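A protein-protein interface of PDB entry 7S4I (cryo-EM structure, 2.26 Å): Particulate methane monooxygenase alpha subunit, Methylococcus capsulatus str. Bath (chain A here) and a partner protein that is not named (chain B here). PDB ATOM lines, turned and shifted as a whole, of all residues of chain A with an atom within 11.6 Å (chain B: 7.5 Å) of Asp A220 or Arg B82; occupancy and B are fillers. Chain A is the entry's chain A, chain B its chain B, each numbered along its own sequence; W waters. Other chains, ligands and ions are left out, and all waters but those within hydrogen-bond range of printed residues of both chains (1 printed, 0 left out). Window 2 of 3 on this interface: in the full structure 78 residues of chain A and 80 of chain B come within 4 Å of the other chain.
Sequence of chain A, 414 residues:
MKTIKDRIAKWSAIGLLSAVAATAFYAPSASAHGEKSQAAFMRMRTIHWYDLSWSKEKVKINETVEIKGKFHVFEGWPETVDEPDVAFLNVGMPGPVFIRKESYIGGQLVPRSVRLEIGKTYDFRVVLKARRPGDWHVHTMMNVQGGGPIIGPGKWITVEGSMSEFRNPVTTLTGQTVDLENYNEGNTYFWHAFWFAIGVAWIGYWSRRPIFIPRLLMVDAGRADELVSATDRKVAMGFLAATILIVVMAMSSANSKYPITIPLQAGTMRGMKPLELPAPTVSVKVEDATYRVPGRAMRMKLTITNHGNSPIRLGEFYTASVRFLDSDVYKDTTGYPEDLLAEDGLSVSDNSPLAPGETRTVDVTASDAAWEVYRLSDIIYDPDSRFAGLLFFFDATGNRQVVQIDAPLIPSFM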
ATOM      1  N   PRO A 210     -11.279  -2.009 -20.351  1.00  0.00           N
ATOM      2  CA  PRO A 210     -12.223  -0.902 -20.152  1.00  0.00           C
ATOM      3  C   PRO A 210     -11.584   0.440 -20.484  1.00  0.00           C
ATOM      4  O   PRO A 210     -10.393   0.655 -20.260  1.00  0.00           O
ATOM      5  CB  PRO A 210     -12.588  -1.008 -18.665  1.00  0.00           C
ATOM      6  CG  PRO A 210     -11.592  -1.965 -18.069  1.00  0.00           C
ATOM      7  CD  PRO A 210     -11.235  -2.892 -19.176  1.00  0.00           C
ATOM      8  N   ILE A 211     -12.396   1.349 -21.027  1.00  0.00           N
ATOM      9  CA  ILE A 211     -11.860   2.511 -21.728  1.00  0.00           C
ATOM     10  C   ILE A 211     -11.948   3.800 -20.919  1.00  0.00           C
ATOM     11  O   ILE A 211     -10.922   4.411 -20.608  1.00  0.00           O
ATOM     12  CB  ILE A 211     -12.564   2.690 -23.085  1.00  0.00           C
ATOM     13  CG1 ILE A 211     -12.444   1.417 -23.922  1.00  0.00           C
ATOM     14  CG2 ILE A 211     -11.987   3.880 -23.834  1.00  0.00           C
ATOM     15  CD1 ILE A 211     -13.406   1.365 -25.083  1.00  0.00           C
ATOM     16  N   PHE A 212     -13.160   4.252 -20.593  1.00  0.00           N
ATOM     17  CA  PHE A 212     -13.326   5.644 -20.181  1.00  0.00           C
ATOM     18  C   PHE A 212     -13.448   5.842 -18.673  1.00  0.00           C
ATOM     19  O   PHE A 212     -12.592   6.490 -18.066  1.00  0.00           O
ATOM     20  CB  PHE A 212     -14.549   6.242 -20.888  1.00  0.00           C
ATOM     21  CG  PHE A 212     -14.300   6.592 -22.323  1.00  0.00           C
ATOM     22  CD1 PHE A 212     -13.392   7.582 -22.658  1.00  0.00           C
ATOM     23  CD2 PHE A 212     -14.969   5.932 -23.338  1.00  0.00           C
ATOM     24  CE1 PHE A 212     -13.157   7.907 -23.977  1.00  0.00           C
ATOM     25  CE2 PHE A 212     -14.738   6.253 -24.660  1.00  0.00           C
ATOM     26  CZ  PHE A 212     -13.832   7.241 -24.980  1.00  0.00           C
ATOM     27  N   ILE A 213     -14.474   5.279 -18.047  1.00  0.00           N
ATOM     28  CA  ILE A 213     -14.807   5.693 -16.685  1.00  0.00           C
ATOM     29  C   ILE A 213     -13.864   5.058 -15.666  1.00  0.00           C
ATOM     30  O   ILE A 213     -13.359   5.775 -14.788  1.00  0.00           O
ATOM     31  CB  ILE A 213     -16.278   5.396 -16.350  1.00  0.00           C
ATOM     32  CG1 ILE A 213     -17.199   6.292 -17.180  1.00  0.00           C
ATOM     33  CG2 ILE A 213     -16.535   5.648 -14.880  1.00  0.00           C
ATOM     34  CD1 ILE A 213     -18.615   6.377 -16.654  1.00  0.00           C
ATOM     35  N   PRO A 214     -13.610   3.741 -15.700  1.00  0.00           N
ATOM     36  CA  PRO A 214     -12.621   3.193 -14.754  1.00  0.00           C
ATOM     37  C   PRO A 214     -11.234   3.788 -14.920  1.00  0.00           C
ATOM     38  O   PRO A 214     -10.552   4.032 -13.917  1.00  0.00           O
ATOM     39  CB  PRO A 214     -12.641   1.687 -15.056  1.00  0.00           C
ATOM     40  CG  PRO A 214     -13.230   1.571 -16.404  1.00  0.00           C
ATOM     41  CD  PRO A 214     -14.222   2.672 -16.508  1.00  0.00           C
ATOM     42  N   ARG A 215     -10.800   4.053 -16.154  1.00  0.00           N
ATOM     43  CA  ARG A 215      -9.489   4.669 -16.348  1.00  0.00           C
ATOM     44  C   ARG A 215      -9.471   6.097 -15.821  1.00  0.00           C
ATOM     45  O   ARG A 215      -8.481   6.529 -15.216  1.00  0.00           O
ATOM     46  CB  ARG A 215      -9.094   4.633 -17.825  1.00  0.00           C
ATOM     47  CG  ARG A 215      -8.718   3.251 -18.331  1.00  0.00           C
ATOM     48  CD  ARG A 215      -8.242   3.283 -19.770  1.00  0.00           C
ATOM     49  NE  ARG A 215      -6.822   3.597 -19.874  1.00  0.00           N
ATOM     50  CZ  ARG A 215      -5.857   2.689 -19.926  1.00  0.00           C
ATOM     51  NH1 ARG A 215      -6.123   1.395 -19.868  1.00  0.00           N
ATOM     52  NH2 ARG A 215      -4.595   3.090 -20.041  1.00  0.00           N
ATOM     53  N   LEU A 216     -10.558   6.843 -16.035  1.00  0.00           N
ATOM     54  CA  LEU A 216     -10.655   8.192 -15.489  1.00  0.00           C
ATOM     55  C   LEU A 216     -10.586   8.172 -13.967  1.00  0.00           C
ATOM     56  O   LEU A 216      -9.886   8.989 -13.358  1.00  0.00           O
ATOM     57  CB  LEU A 216     -11.955   8.844 -15.955  1.00  0.00           C
ATOM     58  CG  LEU A 216     -12.359  10.175 -15.322  1.00  0.00           C
ATOM     59  CD1 LEU A 216     -11.447  11.289 -15.797  1.00  0.00           C
ATOM     60  CD2 LEU A 216     -13.811  10.494 -15.633  1.00  0.00           C
ATOM     61  N   LEU A 217     -11.307   7.239 -13.340  1.00  0.00           N
ATOM     62  CA  LEU A 217     -11.285   7.135 -11.886  1.00  0.00           C
ATOM     63  C   LEU A 217      -9.904   6.741 -11.379  1.00  0.00           C
ATOM     64  O   LEU A 217      -9.447   7.251 -10.351  1.00  0.00           O
ATOM     65  CB  LEU A 217     -12.336   6.131 -11.415  1.00  0.00           C
ATOM     66  CG  LEU A 217     -13.795   6.563 -11.559  1.00  0.00           C
ATOM     67  CD1 LEU A 217     -14.728   5.413 -11.222  1.00  0.00           C
ATOM     68  CD2 LEU A 217     -14.089   7.769 -10.688  1.00  0.00           C
ATOM     69  N   MET A 218      -9.228   5.827 -12.078  1.00  0.00           N
ATOM     70  CA  MET A 218      -7.882   5.436 -11.675  1.00  0.00           C
ATOM     71  C   MET A 218      -6.910   6.604 -11.779  1.00  0.00           C
ATOM     72  O   MET A 218      -6.066   6.794 -10.895  1.00  0.00           O
ATOM     73  CB  MET A 218      -7.399   4.261 -12.523  1.00  0.00           C
ATOM     74  CG  MET A 218      -8.031   2.932 -12.153  1.00  0.00           C
ATOM     75  SD  MET A 218      -7.303   2.222 -10.667  1.00  0.00           S
ATOM     76  CE  MET A 218      -5.646   1.870 -11.246  1.00  0.00           C
ATOM     77  N   VAL A 219      -7.008   7.391 -12.852  1.00  0.00           N
ATOM     78  CA  VAL A 219      -6.114   8.535 -13.010  1.00  0.00           C
ATOM     79  C   VAL A 219      -6.397   9.591 -11.948  1.00  0.00           C
ATOM     80  O   VAL A 219      -5.471  10.170 -11.369  1.00  0.00           O
ATOM     81  CB  VAL A 219      -6.227   9.112 -14.432  1.00  0.00           C
ATOM     82  CG1 VAL A 219      -5.475  10.428 -14.532  1.00  0.00           C
ATOM     83  CG2 VAL A 219      -5.689   8.120 -15.450  1.00  0.00           C
ATOM     84  N   ASP A 220      -7.675   9.855 -11.668  1.00  0.00           N
ATOM     85  CA  ASP A 220      -8.030  10.890 -10.695  1.00  0.00           C
ATOM     86  C   ASP A 220      -7.658  10.475  -9.276  1.00  0.00           C
ATOM     87  O   ASP A 220      -6.891  11.162  -8.594  1.00  0.00           O
ATOM     88  CB  ASP A 220      -9.526  11.210 -10.792  1.00  0.00           C
ATOM     89  CG  ASP A 220      -9.879  11.978 -12.048  1.00  0.00           C
ATOM     90  OD1 ASP A 220      -9.073  12.833 -12.472  1.00  0.00           O
ATOM     91  OD2 ASP A 220     -10.965  11.732 -12.610  1.00  0.00           O
ATOM     92  N   ALA A 221      -8.196   9.347  -8.814  1.00  0.00           N
ATOM     93  CA  ALA A 221      -7.963   8.896  -7.449  1.00  0.00           C
ATOM     94  C   ALA A 221      -6.567   8.309  -7.308  1.00  0.00           C
ATOM     95  O   ALA A 221      -6.357   7.118  -7.559  1.00  0.00           O
ATOM     96  CB  ALA A 221      -9.020   7.871  -7.033  1.00  0.00           C
ATOM     97  N   GLY A 222      -5.610   9.138  -6.905  1.00  0.00           N
ATOM     98  CA  GLY A 222      -4.241   8.701  -6.749  1.00  0.00           C
ATOM     99  C   GLY A 222      -3.504   8.632  -8.070  1.00  0.00           C
ATOM    100  O   GLY A 222      -4.049   8.872  -9.148  1.00  0.00           O
ATOM    101  N   ARG A 223      -2.222   8.294  -7.973  1.00  0.00           N
ATOM    102  CA  ARG A 223      -1.410   8.103  -9.162  1.00  0.00           C
ATOM    103  C   ARG A 223      -1.893   6.872  -9.921  1.00  0.00           C
ATOM    104  O   ARG A 223      -2.266   5.856  -9.330  1.00  0.00           O
ATOM    105  CB  ARG A 223       0.060   7.942  -8.778  1.00  0.00           C
ATOM    106  CG  ARG A 223       0.752   9.241  -8.412  1.00  0.00           C
ATOM    107  CD  ARG A 223       2.151   8.975  -7.888  1.00  0.00           C
ATOM    108  NE  ARG A 223       2.862  10.209  -7.573  1.00  0.00           N
ATOM    109  CZ  ARG A 223       3.693  10.349  -6.550  1.00  0.00           C
ATOM    110  NH1 ARG A 223       3.950   9.346  -5.725  1.00  0.00           N
ATOM    111  NH2 ARG A 223       4.277  11.526  -6.346  1.00  0.00           N
ATOM    112  N   ALA A 224      -1.897   6.967 -11.251  1.00  0.00           N
ATOM    113  CA  ALA A 224      -2.428   5.845 -12.009  1.00  0.00           C
ATOM    114  C   ALA A 224      -1.379   4.755 -12.171  1.00  0.00           C
ATOM    115  O   ALA A 224      -1.473   3.707 -11.524  1.00  0.00           O
ATOM    116  CB  ALA A 224      -2.912   6.316 -13.381  1.00  0.00           C
ATOM    117  N   ASP A 225      -0.373   5.009 -13.008  1.00  0.00           N
ATOM    118  CA  ASP A 225       0.847   4.201 -13.123  1.00  0.00           C
ATOM    119  C   ASP A 225       0.562   2.699 -13.116  1.00  0.00           C
ATOM    120  O   ASP A 225       1.401   1.882 -12.729  1.00  0.00           O
ATOM    121  CB  ASP A 225       1.838   4.568 -12.021  1.00  0.00           C
ATOM    122  CG  ASP A 225       2.470   5.927 -12.238  1.00  0.00           C
ATOM    123  OD1 ASP A 225       2.579   6.353 -13.406  1.00  0.00           O
ATOM    124  OD2 ASP A 225       2.858   6.571 -11.240  1.00  0.00           O
ATOM    125  N   GLU A 226      -0.640   2.328 -13.553  1.00  0.00           N
ATOM    126  CA  GLU A 226      -1.037   0.926 -13.512  1.00  0.00           C
ATOM    127  C   GLU A 226      -1.737   0.509 -14.796  1.00  0.00           C
ATOM    128  O   GLU A 226      -1.762  -0.676 -15.142  1.00  0.00           O
ATOM    129  CB  GLU A 226      -1.940   0.665 -12.305  1.00  0.00           C
ATOM    130  CG  GLU A 226      -1.182   0.413 -11.013  1.00  0.00           C
ATOM    131  CD  GLU A 226      -1.874   1.007  -9.802  1.00  0.00           C
ATOM    132  OE1 GLU A 226      -3.041   0.641  -9.547  1.00  0.00           O
ATOM    133  OE2 GLU A 226      -1.252   1.836  -9.106  1.00  0.00           O
ATOM    134  N   LEU A 227      -2.313   1.477 -15.505  1.00  0.00           N
ATOM    135  CA  LEU A 227      -3.023   1.182 -16.739  1.00  0.00           C
ATOM    136  C   LEU A 227      -2.114   1.192 -17.958  1.00  0.00           C
ATOM    137  O   LEU A 227      -2.543   0.772 -19.039  1.00  0.00           O
ATOM    138  CB  LEU A 227      -4.173   2.173 -16.932  1.00  0.00           C
ATOM    139  CG  LEU A 227      -4.990   2.418 -15.661  1.00  0.00           C
ATOM    140  CD1 LEU A 227      -4.679   3.785 -15.085  1.00  0.00           C
ATOM    141  CD2 LEU A 227      -6.477   2.253 -15.895  1.00  0.00           C
ATOM    142  N   VAL A 228      -0.878   1.661 -17.810  1.00  0.00           N
ATOM    143  CA  VAL A 228       0.117   1.575 -18.871  1.00  0.00           C
ATOM    144  C   VAL A 228       1.354   0.894 -18.301  1.00  0.00           C
ATOM    145  O   VAL A 228       2.205   1.537 -17.678  1.00  0.00           O
ATOM    146  CB  VAL A 228       0.454   2.961 -19.449  1.00  0.00           C
ATOM    147  CG1 VAL A 228       1.593   2.861 -20.453  1.00  0.00           C
ATOM    148  CG2 VAL A 228      -0.775   3.581 -20.094  1.00  0.00           C
ATOM    149  N   GLN B  76      -4.996  14.401 -27.822  1.00  0.00           N
ATOM    150  CA  GLN B  76      -3.971  13.740 -27.025  1.00  0.00           C
ATOM    151  C   GLN B  76      -3.870  14.370 -25.644  1.00  0.00           C
ATOM    152  O   GLN B  76      -3.896  13.668 -24.626  1.00  0.00           O
ATOM    153  CB  GLN B  76      -2.628  13.817 -27.747  1.00  0.00           C
ATOM    154  CG  GLN B  76      -2.236  12.557 -28.481  1.00  0.00           C
ATOM    155  CD  GLN B  76      -0.841  12.647 -29.056  1.00  0.00           C
ATOM    156  OE1 GLN B  76      -0.226  13.712 -29.055  1.00  0.00           O
ATOM    157  NE2 GLN B  76      -0.330  11.526 -29.544  1.00  0.00           N
ATOM    158  N   SER B  77      -3.792  15.705 -25.595  1.00  0.00           N
ATOM    159  CA  SER B  77      -3.668  16.408 -24.323  1.00  0.00           C
ATOM    160  C   SER B  77      -4.836  16.108 -23.401  1.00  0.00           C
ATOM    161  O   SER B  77      -4.708  16.222 -22.178  1.00  0.00           O
ATOM    162  CB  SER B  77      -3.566  17.913 -24.563  1.00  0.00           C
ATOM    163  OG  SER B  77      -4.848  18.515 -24.574  1.00  0.00           O
ATOM    164  N   TYR B  78      -5.984  15.741 -23.964  1.00  0.00           N
ATOM    165  CA  TYR B  78      -7.108  15.356 -23.115  1.00  0.00           C
ATOM    166  C   TYR B  78      -7.068  13.872 -22.762  1.00  0.00           C
ATOM    167  O   TYR B  78      -7.090  13.503 -21.581  1.00  0.00           O
ATOM    168  CB  TYR B  78      -8.423  15.705 -23.802  1.00  0.00           C
ATOM    169  CG  TYR B  78      -9.646  15.097 -23.153  1.00  0.00           C
ATOM    170  CD1 TYR B  78     -10.111  15.561 -21.932  1.00  0.00           C
ATOM    171  CD2 TYR B  78     -10.340  14.064 -23.767  1.00  0.00           C
ATOM    172  CE1 TYR B  78     -11.229  15.013 -21.339  1.00  0.00           C
ATOM    173  CE2 TYR B  78     -11.459  13.509 -23.182  1.00  0.00           C
ATOM    174  CZ  TYR B  78     -11.899  13.987 -21.968  1.00  0.00           C
ATOM    175  OH  TYR B  78     -13.013  13.438 -21.380  1.00  0.00           O
ATOM    176  N   LEU B  79      -7.023  13.007 -23.778  1.00  0.00           N
ATOM    177  CA  LEU B  79      -7.170  11.574 -23.555  1.00  0.00           C
ATOM    178  C   LEU B  79      -6.019  11.018 -22.730  1.00  0.00           C
ATOM    179  O   LEU B  79      -6.242  10.304 -21.749  1.00  0.00           O
ATOM    180  CB  LEU B  79      -7.273  10.842 -24.893  1.00  0.00           C
ATOM    181  CG  LEU B  79      -8.617  10.928 -25.617  1.00  0.00           C
ATOM    182  CD1 LEU B  79      -8.611  10.047 -26.853  1.00  0.00           C
ATOM    183  CD2 LEU B  79      -9.756  10.542 -24.686  1.00  0.00           C
ATOM    184  N   TRP B  80      -4.776  11.326 -23.110  1.00  0.00           N
ATOM    185  CA  TRP B  80      -3.645  10.809 -22.350  1.00  0.00           C
ATOM    186  C   TRP B  80      -3.676  11.319 -20.917  1.00  0.00           C
ATOM    187  O   TRP B  80      -3.564  10.538 -19.966  1.00  0.00           O
ATOM    188  CB  TRP B  80      -2.333  11.186 -23.034  1.00  0.00           C
ATOM    189  CG  TRP B  80      -1.128  10.722 -22.284  1.00  0.00           C
ATOM    190  CD1 TRP B  80      -0.231  11.499 -21.616  1.00  0.00           C
ATOM    191  CD2 TRP B  80      -0.705   9.367 -22.098  1.00  0.00           C
ATOM    192  NE1 TRP B  80       0.737  10.715 -21.038  1.00  0.00           N
ATOM    193  CE2 TRP B  80       0.467   9.401 -21.318  1.00  0.00           C
ATOM    194  CE3 TRP B  80      -1.200   8.130 -22.520  1.00  0.00           C
ATOM    195  CZ2 TRP B  80       1.152   8.247 -20.954  1.00  0.00           C
ATOM    196  CZ3 TRP B  80      -0.518   6.986 -22.156  1.00  0.00           C
ATOM    197  CH2 TRP B  80       0.645   7.052 -21.380  1.00  0.00           C
ATOM    198  N   GLU B  81      -3.895  12.624 -20.743  1.00  0.00           N
ATOM    199  CA  GLU B  81      -3.862  13.211 -19.409  1.00  0.00           C
ATOM    200  C   GLU B  81      -4.948  12.645 -18.504  1.00  0.00           C
ATOM    201  O   GLU B  81      -4.703  12.427 -17.312  1.00  0.00           O
ATOM    202  CB  GLU B  81      -3.994  14.731 -19.501  1.00  0.00           C
ATOM    203  CG  GLU B  81      -3.729  15.476 -18.198  1.00  0.00           C
ATOM    204  CD  GLU B  81      -2.297  15.343 -17.704  1.00  0.00           C
ATOM    205  OE1 GLU B  81      -1.424  14.898 -18.479  1.00  0.00           O
ATOM    206  OE2 GLU B  81      -2.045  15.687 -16.530  1.00  0.00           O
ATOM    207  N   ARG B  82      -6.146  12.397 -19.035  1.00  0.00           N
ATOM    208  CA  ARG B  82      -7.264  12.025 -18.180  1.00  0.00           C
ATOM    209  C   ARG B  82      -7.514  10.524 -18.093  1.00  0.00           C
ATOM    210  O   ARG B  82      -8.130  10.080 -17.119  1.00  0.00           O
ATOM    211  CB  ARG B  82      -8.546  12.720 -18.654  1.00  0.00           C
ATOM    212  CG  ARG B  82      -8.515  14.234 -18.523  1.00  0.00           C
ATOM    213  CD  ARG B  82      -7.968  14.675 -17.171  1.00  0.00           C
ATOM    214  NE  ARG B  82      -8.779  14.190 -16.061  1.00  0.00           N
ATOM    215  CZ  ARG B  82      -9.836  14.825 -15.574  1.00  0.00           C
ATOM    216  NH1 ARG B  82     -10.237  15.982 -16.073  1.00  0.00           N
ATOM    217  NH2 ARG B  82     -10.504  14.288 -14.558  1.00  0.00           N
ATOM    218  N   TYR B  83      -7.062   9.729 -19.067  1.00  0.00           N
ATOM    219  CA  TYR B  83      -7.348   8.303 -19.062  1.00  0.00           C
ATOM    220  C   TYR B  83      -6.135   7.436 -19.360  1.00  0.00           C
ATOM    221  O   TYR B  83      -6.259   6.208 -19.307  1.00  0.00           O
ATOM    222  CB  TYR B  83      -8.447   7.969 -20.087  1.00  0.00           C
ATOM    223  CG  TYR B  83      -9.643   8.895 -20.085  1.00  0.00           C
ATOM    224  CD1 TYR B  83      -9.620  10.097 -20.781  1.00  0.00           C
ATOM    225  CD2 TYR B  83     -10.802   8.559 -19.404  1.00  0.00           C
ATOM    226  CE1 TYR B  83     -10.712  10.940 -20.786  1.00  0.00           C
ATOM    227  CE2 TYR B  83     -11.898   9.394 -19.405  1.00  0.00           C
ATOM    228  CZ  TYR B  83     -11.847  10.584 -20.096  1.00  0.00           C
ATOM    229  OH  TYR B  83     -12.940  11.418 -20.097  1.00  0.00           O
ATOM    230  N   ARG B  84      -4.975   8.020 -19.670  1.00  0.00           N
ATOM    231  CA  ARG B  84      -3.817   7.272 -20.157  1.00  0.00           C
ATOM    232  C   ARG B  84      -4.181   6.432 -21.378  1.00  0.00           C
ATOM    233  O   ARG B  84      -3.765   5.280 -21.516  1.00  0.00           O
ATOM    234  CB  ARG B  84      -3.207   6.409 -19.052  1.00  0.00           C
ATOM    235  CG  ARG B  84      -2.574   7.214 -17.936  1.00  0.00           C
ATOM    236  CD  ARG B  84      -1.241   7.796 -18.375  1.00  0.00           C
ATOM    237  NE  ARG B  84      -0.658   8.679 -17.373  1.00  0.00           N
ATOM    238  CZ  ARG B  84      -1.129   9.878 -17.058  1.00  0.00           C
ATOM    239  NH1 ARG B  84      -2.187  10.389 -17.666  1.00  0.00           N
ATOM    240  NH2 ARG B  84      -0.519  10.585 -16.111  1.00  0.00           N
ATOM    241  N   LEU B  85      -4.974   7.019 -22.275  1.00  0.00           N
ATOM    242  CA  LEU B  85      -5.330   6.383 -23.539  1.00  0.00           C
ATOM    243  C   LEU B  85      -4.473   6.986 -24.642  1.00  0.00           C
ATOM    244  O   LEU B  85      -4.702   8.136 -25.048  1.00  0.00           O
ATOM    245  CB  LEU B  85      -6.816   6.580 -23.848  1.00  0.00           C
ATOM    246  CG  LEU B  85      -7.794   5.734 -23.036  1.00  0.00           C
ATOM    247  CD1 LEU B  85      -9.214   6.228 -23.240  1.00  0.00           C
ATOM    248  CD2 LEU B  85      -7.676   4.271 -23.414  1.00  0.00           C
ATOM    249  N   TYR B 141       4.797  15.772 -22.680  1.00  0.00           N
ATOM    250  CA  TYR B 141       4.136  16.477 -23.772  1.00  0.00           C
ATOM    251  C   TYR B 141       5.109  17.355 -24.546  1.00  0.00           C
ATOM    252  O   TYR B 141       4.964  17.507 -25.763  1.00  0.00           O
ATOM    253  CB  TYR B 141       2.975  17.316 -23.238  1.00  0.00           C
ATOM    254  CG  TYR B 141       1.747  16.511 -22.889  1.00  0.00           C
ATOM    255  CD1 TYR B 141       0.954  15.954 -23.883  1.00  0.00           C
ATOM    256  CD2 TYR B 141       1.379  16.307 -21.567  1.00  0.00           C
ATOM    257  CE1 TYR B 141      -0.169  15.220 -23.571  1.00  0.00           C
ATOM    258  CE2 TYR B 141       0.260  15.573 -21.245  1.00  0.00           C
ATOM    259  CZ  TYR B 141      -0.512  15.033 -22.249  1.00  0.00           C
ATOM    260  OH  TYR B 141      -1.629  14.301 -21.928  1.00  0.00           O
ATOM    261  N   ARG B 236      -6.249  21.657 -23.727  1.00  0.00           N
ATOM    262  CA  ARG B 236      -6.321  21.804 -22.278  1.00  0.00           C
ATOM    263  C   ARG B 236      -7.479  22.709 -21.883  1.00  0.00           C
ATOM    264  O   ARG B 236      -8.248  22.393 -20.969  1.00  0.00           O
ATOM    265  CB  ARG B 236      -5.001  22.357 -21.740  1.00  0.00           C
ATOM    266  CG  ARG B 236      -3.973  21.295 -21.412  1.00  0.00           C
ATOM    267  CD  ARG B 236      -4.590  20.172 -20.603  1.00  0.00           C
ATOM    268  NE  ARG B 236      -3.980  18.886 -20.913  1.00  0.00           N
ATOM    269  CZ  ARG B 236      -2.821  18.470 -20.424  1.00  0.00           C
ATOM    270  NH1 ARG B 236      -2.121  19.208 -19.580  1.00  0.00           N
ATOM    271  NH2 ARG B 236      -2.353  17.281 -20.791  1.00  0.00           N
ATOM    272  N   SER B 239     -11.008  21.186 -22.444  1.00  0.00           N
ATOM    273  CA  SER B 239     -11.363  20.114 -21.478  1.00  0.00           C
ATOM    274  C   SER B 239     -12.003  20.711 -20.218  1.00  0.00           C
ATOM    275  O   SER B 239     -12.615  19.940 -19.476  1.00  0.00           O
ATOM    276  CB  SER B 239     -10.151  19.289 -21.141  1.00  0.00           C
ATOM    277  OG  SER B 239      -9.664  18.618 -22.290  1.00  0.00           O
ATOM    278  N   ASN B 240     -11.903  22.028 -20.008  1.00  0.00           N
ATOM    279  CA  ASN B 240     -12.428  22.694 -18.778  1.00  0.00           C
ATOM    280  C   ASN B 240     -13.780  22.109 -18.345  1.00  0.00           C
ATOM    281  O   ASN B 240     -14.660  21.934 -19.207  1.00  0.00           O
ATOM    282  CB  ASN B 240     -12.466  24.222 -18.932  1.00  0.00           C
ATOM    283  CG  ASN B 240     -13.756  24.764 -19.513  1.00  0.00           C
ATOM    284  OD1 ASN B 240     -14.669  25.125 -18.775  1.00  0.00           O
ATOM    285  ND2 ASN B 240     -13.843  24.825 -20.832  1.00  0.00           N
ATOM    286  N   GLU B 241     -13.932  21.808 -17.052  1.00  0.00           N
ATOM    287  CA  GLU B 241     -15.200  21.316 -16.522  1.00  0.00           C
ATOM    288  C   GLU B 241     -15.901  22.394 -15.708  1.00  0.00           C
ATOM    289  O   GLU B 241     -16.607  22.105 -14.738  1.00  0.00           O
ATOM    290  CB  GLU B 241     -14.988  20.065 -15.675  1.00  0.00           C
ATOM    291  CG  GLU B 241     -14.270  18.940 -16.391  1.00  0.00           C
ATOM    292  CD  GLU B 241     -13.264  18.236 -15.502  1.00  0.00           C
ATOM    293  OE1 GLU B 241     -13.572  18.009 -14.314  1.00  0.00           O
ATOM    294  OE2 GLU B 241     -12.162  17.911 -15.991  1.00  0.00           O
HETATM  295  O   HOH W   1      -8.334  11.756 -14.678  1.00  0.00           O
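Of the printed residues of chain B, Phe A212 touches Tyr B83. Of the printed residues of chain B, Leu A216 touches Arg B82 and Tyr B83. Glu A226 touches none of the printed residues of chain B. Glu B81 touches one residue of chain A. Of chain A, only Leu A216 (3.4 Å), Val A219 (3.4 Å) and Asp A220 (2.9 Å) come within 4 Å of Arg B82. Tyr B83 touches just these residues of chain A: Phe A212, Arg A215, Leu A216 and Val A219. Of chain A, only Arg A215 (2.8 Å) and Val A228 (3.7 Å) come within 4 Å of Arg B84. The nearest residue of chain A that does not touch Arg B82 is Arg A215 (4.04 Å).
Water W1 lies within hydrogen-bond range of the side-chain carboxylate (OD1) of Asp A220 (2.6 Å), the guanidinium group (NE) of Arg B82 (2.8 Å) and the backbone carbonyl oxygen (O) of Leu A216 (3.4 Å).
O of Ile A211 touches CD1 of Leu B85 (3.6 Å). CD2 of Tyr B83 touches O of Phe A212, 3.0 Å away. NE of Arg A215 touches CD2 of Leu B85, at 3.7 Å. CD1 of Leu A216 touches NH2 of Arg B82, at 3.4 Å. Tyr B83 touches Leu A216. Val A219 touches Glu B81 (CG1 to O, 3.5 Å). CB of Val A219 touches O of Arg B82, at 3.4 Å. Val A219 touches Tyr B83 (CG2 to CA, 3.98 Å). CG2 of Val A228 touches CH2 of Trp B80, at 3.96 Å. Arg B84 touches Val A228 (O to CG2, 3.7 Å).
The guanidinium group (NH2) of Arg A215 lies within hydrogen-bond range of the backbone carbonyl oxygen (O) of Leu A227, 3.3 Å away. The guanidinium group of Arg B84 is in hydrogen-bond range of the backbone carbonyl oxygen of Trp B80 (2.7 Å). The backbone carbonyl oxygen (O) of Glu B81 lies within hydrogen-bond range of the guanidinium group (NH1) of Arg B84 (3.3 Å). The backbone NH (N) of Glu B81 sits at hydrogen-bond distance from the side-chain hydroxyl (OH) of Tyr B141 (3.1 Å). The guanidinium group of Arg B236 is in salt-bridge range of the side-chain carboxylate of Glu B81, 3.4 Å away. The side-chain carboxylate of Glu B241 lies within salt-bridge range of the guanidinium group of Arg B82 (2.7 Å).
Of the 19 printed residues of chain A, 7 touch a printed residue of chain B. Hydrophobic or aromatic side chains of chain A within 4 Å of the printed part of chain B: Ile A211, Leu A216, Val A219 and Val A228. Hydrophobic or aromatic side chains of chain B that line the printed part of chain A: Trp B80, Tyr B83 and Leu B85.
The guanidinium group (NE) of Arg A215 sits at hydrogen-bond distance from the backbone carbonyl oxygen (O) of Tyr B83 (2.7 Å). The backbone carbonyl oxygen of Arg B84 is in hydrogen-bond range of the guanidinium group of Arg A215 (2.8 Å). The side-chain carboxylate (OD1) of Asp A220 lies within salt-bridge range of the guanidinium group (NH2) of Arg B82, at 2.9 Å.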
